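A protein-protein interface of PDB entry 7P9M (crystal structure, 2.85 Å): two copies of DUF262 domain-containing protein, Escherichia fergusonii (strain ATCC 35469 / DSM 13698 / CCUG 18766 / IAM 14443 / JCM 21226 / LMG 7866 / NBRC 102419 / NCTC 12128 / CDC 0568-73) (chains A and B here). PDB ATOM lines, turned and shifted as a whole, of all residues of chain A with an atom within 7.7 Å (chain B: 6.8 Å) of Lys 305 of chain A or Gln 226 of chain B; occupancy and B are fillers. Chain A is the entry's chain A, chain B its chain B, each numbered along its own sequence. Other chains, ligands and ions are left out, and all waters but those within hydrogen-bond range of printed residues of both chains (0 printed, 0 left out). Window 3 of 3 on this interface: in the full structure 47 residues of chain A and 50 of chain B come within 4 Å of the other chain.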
ATOM      1  N   TYR A 247     -13.859  22.943  37.012  1.00  0.00           N
ATOM      2  CA  TYR A 247     -14.203  22.722  35.592  1.00  0.00           C
ATOM      3  C   TYR A 247     -15.565  22.028  35.599  1.00  0.00           C
ATOM      4  O   TYR A 247     -15.638  20.843  35.271  1.00  0.00           O
ATOM      5  CB  TYR A 247     -13.067  22.013  34.860  1.00  0.00           C
ATOM      6  CG  TYR A 247     -12.734  22.571  33.502  1.00  0.00           C
ATOM      7  CD1 TYR A 247     -12.624  23.933  33.293  1.00  0.00           C
ATOM      8  CD2 TYR A 247     -12.524  21.732  32.425  1.00  0.00           C
ATOM      9  CE1 TYR A 247     -12.320  24.447  32.044  1.00  0.00           C
ATOM     10  CE2 TYR A 247     -12.221  22.228  31.171  1.00  0.00           C
ATOM     11  CZ  TYR A 247     -12.118  23.592  30.979  1.00  0.00           C
ATOM     12  OH  TYR A 247     -11.816  24.076  29.743  1.00  0.00           O
ATOM     13  N   ASP A 249     -18.177  21.425  33.773  1.00  0.00           N
ATOM     14  CA  ASP A 249     -18.707  21.396  32.394  1.00  0.00           C
ATOM     15  C   ASP A 249     -20.042  20.678  32.477  1.00  0.00           C
ATOM     16  O   ASP A 249     -20.671  20.473  31.442  1.00  0.00           O
ATOM     17  CB  ASP A 249     -17.768  20.615  31.483  1.00  0.00           C
ATOM     18  CG  ASP A 249     -16.336  21.102  31.491  1.00  0.00           C
ATOM     19  OD1 ASP A 249     -16.082  22.162  32.079  1.00  0.00           O
ATOM     20  OD2 ASP A 249     -15.494  20.414  30.897  1.00  0.00           O
ATOM     21  N   LEU A 252     -22.646  22.979  31.397  1.00  0.00           N
ATOM     22  CA  LEU A 252     -22.801  23.169  29.943  1.00  0.00           C
ATOM     23  C   LEU A 252     -23.795  22.137  29.454  1.00  0.00           C
ATOM     24  O   LEU A 252     -24.316  22.295  28.356  1.00  0.00           O
ATOM     25  CB  LEU A 252     -21.437  22.965  29.291  1.00  0.00           C
ATOM     26  CG  LEU A 252     -20.522  24.188  29.240  1.00  0.00           C
ATOM     27  CD1 LEU A 252     -19.919  24.503  30.602  1.00  0.00           C
ATOM     28  CD2 LEU A 252     -19.416  23.980  28.223  1.00  0.00           C
ATOM     29  N   LYS A 291     -16.444  11.848  31.319  1.00  0.00           N
ATOM     30  CA  LYS A 291     -15.366  11.450  30.392  1.00  0.00           C
ATOM     31  C   LYS A 291     -15.815  10.169  29.730  1.00  0.00           C
ATOM     32  O   LYS A 291     -15.605  10.005  28.540  1.00  0.00           O
ATOM     33  CB  LYS A 291     -14.061  11.244  31.154  1.00  0.00           C
ATOM     34  CG  LYS A 291     -12.810  11.246  30.290  1.00  0.00           C
ATOM     35  CD  LYS A 291     -12.096  12.570  30.268  1.00  0.00           C
ATOM     36  CE  LYS A 291     -10.760  12.498  29.560  1.00  0.00           C
ATOM     37  NZ  LYS A 291      -9.623  12.520  30.510  1.00  0.00           N
ATOM     38  N   LEU A 294     -18.082  10.619  26.673  1.00  0.00           N
ATOM     39  CA  LEU A 294     -17.508  10.746  25.327  1.00  0.00           C
ATOM     40  C   LEU A 294     -16.869   9.425  24.941  1.00  0.00           C
ATOM     41  O   LEU A 294     -16.906   9.076  23.763  1.00  0.00           O
ATOM     42  CB  LEU A 294     -16.474  11.869  25.388  1.00  0.00           C
ATOM     43  CG  LEU A 294     -16.901  13.123  26.142  1.00  0.00           C
ATOM     44  CD1 LEU A 294     -15.681  13.912  26.573  1.00  0.00           C
ATOM     45  CD2 LEU A 294     -17.802  13.990  25.281  1.00  0.00           C
ATOM     46  N   SER A 301     -13.092  12.566  20.214  1.00  0.00           N
ATOM     47  CA  SER A 301     -12.200  13.276  21.162  1.00  0.00           C
ATOM     48  C   SER A 301     -12.690  13.079  22.591  1.00  0.00           C
ATOM     49  O   SER A 301     -13.816  13.481  22.878  1.00  0.00           O
ATOM     50  CB  SER A 301     -12.123  14.719  20.831  1.00  0.00           C
ATOM     51  OG  SER A 301     -11.389  15.418  21.823  1.00  0.00           O
ATOM     52  N   VAL A 302     -11.841  12.536  23.460  1.00  0.00           N
ATOM     53  CA  VAL A 302     -12.281  12.196  24.842  1.00  0.00           C
ATOM     54  C   VAL A 302     -11.875  13.296  25.807  1.00  0.00           C
ATOM     55  O   VAL A 302     -12.204  13.170  26.968  1.00  0.00           O
ATOM     56  CB  VAL A 302     -11.666  10.859  25.269  1.00  0.00           C
ATOM     57  CG1 VAL A 302     -11.994  10.542  26.714  1.00  0.00           C
ATOM     58  CG2 VAL A 302     -12.119   9.727  24.367  1.00  0.00           C
ATOM     59  N   GLY A 303     -11.267  14.369  25.327  1.00  0.00           N
ATOM     60  CA  GLY A 303     -10.786  15.434  26.223  1.00  0.00           C
ATOM     61  C   GLY A 303     -11.863  15.961  27.147  1.00  0.00           C
ATOM     62  O   GLY A 303     -13.015  16.056  26.720  1.00  0.00           O
ATOM     63  N   PHE A 304     -11.487  16.297  28.382  1.00  0.00           N
ATOM     64  CA  PHE A 304     -12.442  16.884  29.351  1.00  0.00           C
ATOM     65  C   PHE A 304     -12.505  18.378  29.066  1.00  0.00           C
ATOM     66  O   PHE A 304     -12.931  19.155  29.916  1.00  0.00           O
ATOM     67  CB  PHE A 304     -11.982  16.622  30.783  1.00  0.00           C
ATOM     68  CG  PHE A 304     -13.074  16.671  31.814  1.00  0.00           C
ATOM     69  CD1 PHE A 304     -14.221  15.915  31.663  1.00  0.00           C
ATOM     70  CD2 PHE A 304     -12.957  17.485  32.926  1.00  0.00           C
ATOM     71  CE1 PHE A 304     -15.226  15.968  32.612  1.00  0.00           C
ATOM     72  CE2 PHE A 304     -13.965  17.538  33.873  1.00  0.00           C
ATOM     73  CZ  PHE A 304     -15.098  16.780  33.713  1.00  0.00           C
ATOM     74  N   LYS A 305     -12.120  18.755  27.858  1.00  0.00           N
ATOM     75  CA  LYS A 305     -12.160  20.179  27.479  1.00  0.00           C
ATOM     76  C   LYS A 305     -13.604  20.591  27.216  1.00  0.00           C
ATOM     77  O   LYS A 305     -14.405  19.720  26.895  1.00  0.00           O
ATOM     78  CB  LYS A 305     -11.304  20.357  26.228  1.00  0.00           C
ATOM     79  CG  LYS A 305      -9.814  20.130  26.418  1.00  0.00           C
ATOM     80  CD  LYS A 305      -9.035  20.299  25.137  1.00  0.00           C
ATOM     81  CE  LYS A 305      -7.547  20.097  25.325  1.00  0.00           C
ATOM     82  NZ  LYS A 305      -6.813  20.246  24.047  1.00  0.00           N
ATOM     83  N   VAL A 306     -13.898  21.889  27.257  1.00  0.00           N
ATOM     84  CA  VAL A 306     -15.280  22.399  27.027  1.00  0.00           C
ATOM     85  C   VAL A 306     -15.614  22.297  25.546  1.00  0.00           C
ATOM     86  O   VAL A 306     -16.782  22.435  25.201  1.00  0.00           O
ATOM     87  CB  VAL A 306     -15.411  23.851  27.501  1.00  0.00           C
ATOM     88  CG1 VAL A 306     -15.347  23.953  29.013  1.00  0.00           C
ATOM     89  CG2 VAL A 306     -14.363  24.747  26.864  1.00  0.00           C
ATOM     90  N   GLU A 307     -14.619  22.053  24.706  1.00  0.00           N
ATOM     91  CA  GLU A 307     -14.861  22.038  23.244  1.00  0.00           C
ATOM     92  C   GLU A 307     -15.709  20.826  22.893  1.00  0.00           C
ATOM     93  O   GLU A 307     -16.556  20.938  22.002  1.00  0.00           O
ATOM     94  CB  GLU A 307     -13.529  21.964  22.501  1.00  0.00           C
ATOM     95  CG  GLU A 307     -13.635  22.226  21.010  1.00  0.00           C
ATOM     96  CD  GLU A 307     -14.388  23.485  20.620  1.00  0.00           C
ATOM     97  OE1 GLU A 307     -13.875  24.586  20.883  1.00  0.00           O
ATOM     98  OE2 GLU A 307     -15.482  23.363  20.044  1.00  0.00           O
ATOM     99  N   ASN A 308     -15.477  19.704  23.572  1.00  0.00           N
ATOM    100  CA  ASN A 308     -16.166  18.437  23.227  1.00  0.00           C
ATOM    101  C   ASN A 308     -17.499  18.352  23.954  1.00  0.00           C
ATOM    102  O   ASN A 308     -18.158  17.332  23.827  1.00  0.00           O
ATOM    103  CB  ASN A 308     -15.279  17.244  23.559  1.00  0.00           C
ATOM    104  CG  ASN A 308     -13.881  17.393  23.007  1.00  0.00           C
ATOM    105  OD1 ASN A 308     -13.703  17.752  21.848  1.00  0.00           O
ATOM    106  ND2 ASN A 308     -12.885  17.122  23.830  1.00  0.00           N
ATOM    107  N   PHE A 309     -17.835  19.368  24.736  1.00  0.00           N
ATOM    108  CA  PHE A 309     -19.103  19.363  25.496  1.00  0.00           C
ATOM    109  C   PHE A 309     -20.080  20.220  24.718  1.00  0.00           C
ATOM    110  O   PHE A 309     -20.907  20.909  25.313  1.00  0.00           O
ATOM    111  CB  PHE A 309     -18.866  19.809  26.932  1.00  0.00           C
ATOM    112  CG  PHE A 309     -18.395  18.705  27.840  1.00  0.00           C
ATOM    113  CD1 PHE A 309     -17.171  18.091  27.638  1.00  0.00           C
ATOM    114  CD2 PHE A 309     -19.183  18.264  28.887  1.00  0.00           C
ATOM    115  CE1 PHE A 309     -16.741  17.071  28.468  1.00  0.00           C
ATOM    116  CE2 PHE A 309     -18.753  17.243  29.716  1.00  0.00           C
ATOM    117  CZ  PHE A 309     -17.534  16.648  29.505  1.00  0.00           C
ATOM    118  N   ASN A 310     -20.005  20.132  23.392  1.00  0.00           N
ATOM    119  CA  ASN A 310     -20.848  20.989  22.524  1.00  0.00           C
ATOM    120  C   ASN A 310     -22.279  20.480  22.476  1.00  0.00           C
ATOM    121  O   ASN A 310     -22.496  19.340  22.836  1.00  0.00           O
ATOM    122  CB  ASN A 310     -20.265  21.169  21.124  1.00  0.00           C
ATOM    123  CG  ASN A 310     -20.140  19.914  20.300  1.00  0.00           C
ATOM    124  OD1 ASN A 310     -20.265  18.821  20.825  1.00  0.00           O
ATOM    125  ND2 ASN A 310     -19.962  20.057  19.003  1.00  0.00           N
ATOM    126  N   MET A 314     -23.154  16.657  22.979  1.00  0.00           N
ATOM    127  CA  MET A 314     -23.974  16.280  24.154  1.00  0.00           C
ATOM    128  C   MET A 314     -25.310  15.762  23.674  1.00  0.00           C
ATOM    129  O   MET A 314     -26.080  15.377  24.516  1.00  0.00           O
ATOM    130  CB  MET A 314     -24.242  17.471  25.071  1.00  0.00           C
ATOM    131  CG  MET A 314     -23.026  18.029  25.746  1.00  0.00           C
ATOM    132  SD  MET A 314     -22.409  16.908  26.991  1.00  0.00           S
ATOM    133  CE  MET A 314     -20.870  16.422  26.219  1.00  0.00           C
ATOM    134  N   ASP A 400      -5.750  10.686  27.364  1.00  0.00           N
ATOM    135  CA  ASP A 400      -6.767  10.905  26.318  1.00  0.00           C
ATOM    136  C   ASP A 400      -6.336  10.157  25.062  1.00  0.00           C
ATOM    137  O   ASP A 400      -7.203   9.740  24.307  1.00  0.00           O
ATOM    138  CB  ASP A 400      -7.013  12.398  26.152  1.00  0.00           C
ATOM    139  CG  ASP A 400      -7.753  12.979  27.340  1.00  0.00           C
ATOM    140  OD1 ASP A 400      -8.305  12.186  28.120  1.00  0.00           O
ATOM    141  OD2 ASP A 400      -7.747  14.216  27.486  1.00  0.00           O
ATOM    142  N   TRP B  55     -15.191  34.198  30.171  1.00  0.00           N
ATOM    143  CA  TRP B  55     -14.892  33.225  29.088  1.00  0.00           C
ATOM    144  C   TRP B  55     -15.325  33.802  27.752  1.00  0.00           C
ATOM    145  O   TRP B  55     -16.511  34.028  27.573  1.00  0.00           O
ATOM    146  CB  TRP B  55     -15.597  31.896  29.352  1.00  0.00           C
ATOM    147  CG  TRP B  55     -15.542  30.901  28.237  1.00  0.00           C
ATOM    148  CD1 TRP B  55     -14.537  30.696  27.337  1.00  0.00           C
ATOM    149  CD2 TRP B  55     -16.558  29.938  27.924  1.00  0.00           C
ATOM    150  NE1 TRP B  55     -14.867  29.688  26.475  1.00  0.00           N
ATOM    151  CE2 TRP B  55     -16.101  29.203  26.813  1.00  0.00           C
ATOM    152  CE3 TRP B  55     -17.806  29.636  28.471  1.00  0.00           C
ATOM    153  CZ2 TRP B  55     -16.853  28.181  26.243  1.00  0.00           C
ATOM    154  CZ3 TRP B  55     -18.549  28.626  27.908  1.00  0.00           C
ATOM    155  CH2 TRP B  55     -18.076  27.910  26.810  1.00  0.00           C
ATOM    156  N   LYS B  58     -15.631  31.934  21.004  1.00  0.00           N
ATOM    157  CA  LYS B  58     -15.247  32.193  19.602  1.00  0.00           C
ATOM    158  C   LYS B  58     -16.515  32.267  18.763  1.00  0.00           C
ATOM    159  O   LYS B  58     -17.509  31.656  19.142  1.00  0.00           O
ATOM    160  CB  LYS B  58     -14.355  31.050  19.123  1.00  0.00           C
ATOM    161  CG  LYS B  58     -12.874  31.377  19.000  1.00  0.00           C
ATOM    162  CD  LYS B  58     -12.031  30.157  18.710  1.00  0.00           C
ATOM    163  CE  LYS B  58     -10.638  30.498  18.228  1.00  0.00           C
ATOM    164  NZ  LYS B  58      -9.651  29.483  18.659  1.00  0.00           N
ATOM    165  N   GLU B 223     -10.423  34.503  28.723  1.00  0.00           N
ATOM    166  CA  GLU B 223      -9.659  33.504  27.926  1.00  0.00           C
ATOM    167  C   GLU B 223     -10.569  32.769  26.940  1.00  0.00           C
ATOM    168  O   GLU B 223     -11.783  32.960  27.017  1.00  0.00           O
ATOM    169  CB  GLU B 223      -8.841  32.533  28.761  1.00  0.00           C
ATOM    170  CG  GLU B 223      -8.020  31.577  27.911  1.00  0.00           C
ATOM    171  CD  GLU B 223      -6.919  32.190  27.061  1.00  0.00           C
ATOM    172  OE1 GLU B 223      -6.585  33.370  27.285  1.00  0.00           O
ATOM    173  OE2 GLU B 223      -6.402  31.489  26.173  1.00  0.00           O
ATOM    174  N   SER B 224      -9.988  31.936  26.074  1.00  0.00           N
ATOM    175  CA  SER B 224     -10.780  31.274  25.007  1.00  0.00           C
ATOM    176  C   SER B 224     -10.927  29.791  25.297  1.00  0.00           C
ATOM    177  O   SER B 224     -10.214  29.330  26.157  1.00  0.00           O
ATOM    178  CB  SER B 224     -10.105  31.454  23.698  1.00  0.00           C
ATOM    179  OG  SER B 224      -9.073  30.492  23.538  1.00  0.00           O
ATOM    180  N   ASP B 225     -11.691  29.065  24.492  1.00  0.00           N
ATOM    181  CA  ASP B 225     -11.957  27.623  24.714  1.00  0.00           C
ATOM    182  C   ASP B 225     -10.693  26.807  24.981  1.00  0.00           C
ATOM    183  O   ASP B 225     -10.655  26.111  26.005  1.00  0.00           O
ATOM    184  CB  ASP B 225     -12.615  27.004  23.482  1.00  0.00           C
ATOM    185  CG  ASP B 225     -11.818  27.045  22.190  1.00  0.00           C
ATOM    186  OD1 ASP B 225     -10.725  27.637  22.179  1.00  0.00           O
ATOM    187  OD2 ASP B 225     -12.295  26.460  21.200  1.00  0.00           O
ATOM    188  N   GLN B 226      -9.710  26.870  24.092  1.00  0.00           N
ATOM    189  CA  GLN B 226      -8.519  25.996  24.230  1.00  0.00           C
ATOM    190  C   GLN B 226      -7.875  26.153  25.598  1.00  0.00           C
ATOM    191  O   GLN B 226      -7.846  25.171  26.346  1.00  0.00           O
ATOM    192  CB  GLN B 226      -7.480  26.343  23.168  1.00  0.00           C
ATOM    193  CG  GLN B 226      -6.357  25.324  23.058  1.00  0.00           C
ATOM    194  CD  GLN B 226      -6.799  24.092  22.309  1.00  0.00           C
ATOM    195  OE1 GLN B 226      -6.717  22.974  22.809  1.00  0.00           O
ATOM    196  NE2 GLN B 226      -7.279  24.295  21.093  1.00  0.00           N
ATOM    197  N   SER B 227      -7.424  27.356  25.927  1.00  0.00           N
ATOM    198  CA  SER B 227      -6.648  27.511  27.178  1.00  0.00           C
ATOM    199  C   SER B 227      -7.503  27.918  28.368  1.00  0.00           C
ATOM    200  O   SER B 227      -6.903  28.202  29.389  1.00  0.00           O
ATOM    201  CB  SER B 227      -5.537  28.475  26.981  1.00  0.00           C
ATOM    202  OG  SER B 227      -4.603  27.963  26.044  1.00  0.00           O
ATOM    203  N   LEU B 228      -8.823  27.801  28.286  1.00  0.00           N
ATOM    204  CA  LEU B 228      -9.666  28.110  29.465  1.00  0.00           C
ATOM    205  C   LEU B 228      -9.278  27.198  30.618  1.00  0.00           C
ATOM    206  O   LEU B 228      -9.318  27.639  31.759  1.00  0.00           O
ATOM    207  CB  LEU B 228     -11.132  27.909  29.091  1.00  0.00           C
ATOM    208  CG  LEU B 228     -12.144  28.355  30.138  1.00  0.00           C
ATOM    209  CD1 LEU B 228     -12.045  29.850  30.372  1.00  0.00           C
ATOM    210  CD2 LEU B 228     -13.550  27.972  29.719  1.00  0.00           C
ATOM    211  N   GLU B 229      -8.852  25.985  30.320  1.00  0.00           N
ATOM    212  CA  GLU B 229      -8.563  25.026  31.406  1.00  0.00           C
ATOM    213  C   GLU B 229      -7.475  25.591  32.296  1.00  0.00           C
ATOM    214  O   GLU B 229      -7.689  25.682  33.506  1.00  0.00           O
ATOM    215  CB  GLU B 229      -8.031  23.739  30.792  1.00  0.00           C
ATOM    216  CG  GLU B 229      -7.762  22.643  31.807  1.00  0.00           C
ATOM    217  CD  GLU B 229      -7.275  21.321  31.239  1.00  0.00           C
ATOM    218  OE1 GLU B 229      -7.095  21.238  30.012  1.00  0.00           O
ATOM    219  OE2 GLU B 229      -7.091  20.377  32.024  1.00  0.00           O
ATOM    220  N   ARG B 230      -6.371  26.002  31.692  1.00  0.00           N
ATOM    221  CA  ARG B 230      -5.210  26.479  32.477  1.00  0.00           C
ATOM    222  C   ARG B 230      -5.561  27.700  33.302  1.00  0.00           C
ATOM    223  O   ARG B 230      -5.249  27.708  34.489  1.00  0.00           O
ATOM    224  CB  ARG B 230      -4.149  27.011  31.522  1.00  0.00           C
ATOM    225  CG  ARG B 230      -2.884  27.515  32.196  1.00  0.00           C
ATOM    226  CD  ARG B 230      -1.909  27.936  31.115  1.00  0.00           C
ATOM    227  NE  ARG B 230      -2.433  29.073  30.371  1.00  0.00           N
ATOM    228  CZ  ARG B 230      -2.334  30.338  30.758  1.00  0.00           C
ATOM    229  NH1 ARG B 230      -1.728  30.637  31.894  1.00  0.00           N
ATOM    230  NH2 ARG B 230      -2.843  31.299  30.010  1.00  0.00           N
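The side-chain carboxylate (OD2) of Asp 225 of chain B lies close to the side-chain carboxylate (OE1) of Glu 307 of chain A, 2.5 Å away.
NZ of Lys 305 of chain A is in hydrogen-bond range of OE1 of Gln 226 of chain B (3.0 Å).
No position is printed for both chains.
Among the printed residues, merely in contact across the chains: Tyr 247 of chain A with Leu 228 of chain B (3.9 Å) and Tyr 247 of chain A with Glu 229 of chain B (3.6 Å).
Of the 17 printed residues of chain A, 3 touch a printed residue of chain B.
Printed residues of chain B that touch a printed residue of chain A: Asp 225, Gln 226, Leu 228 and Glu 229.
Hydrophobic or aromatic side chains of chain B that line the printed part of chain A: Leu 228.
Among the printed residues, 4 pairs touch across the chains.
Among the printed residues, no Asp or Glu carboxylate lies within 4 Å of a Lys or Arg side-chain nitrogen of the other chain.
Printed residues of chain B within 4 Å of Tyr 247 of chain A: Leu 228 (3.9 Å) and Glu 229 (3.6 Å).
Of the printed residues of chain A, Asp 225 of chain B touches Glu 307 (2.5 Å).
Gln 226 of chain B touches just one residue of chain A: Lys 305.
Of the printed residues of chain A, Leu 228 of chain B touches Tyr 247 (3.9 Å).
The nearest residue of chain A that does not touch Gln 226 of chain B is Tyr 247 of chain A (5.3 Å).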
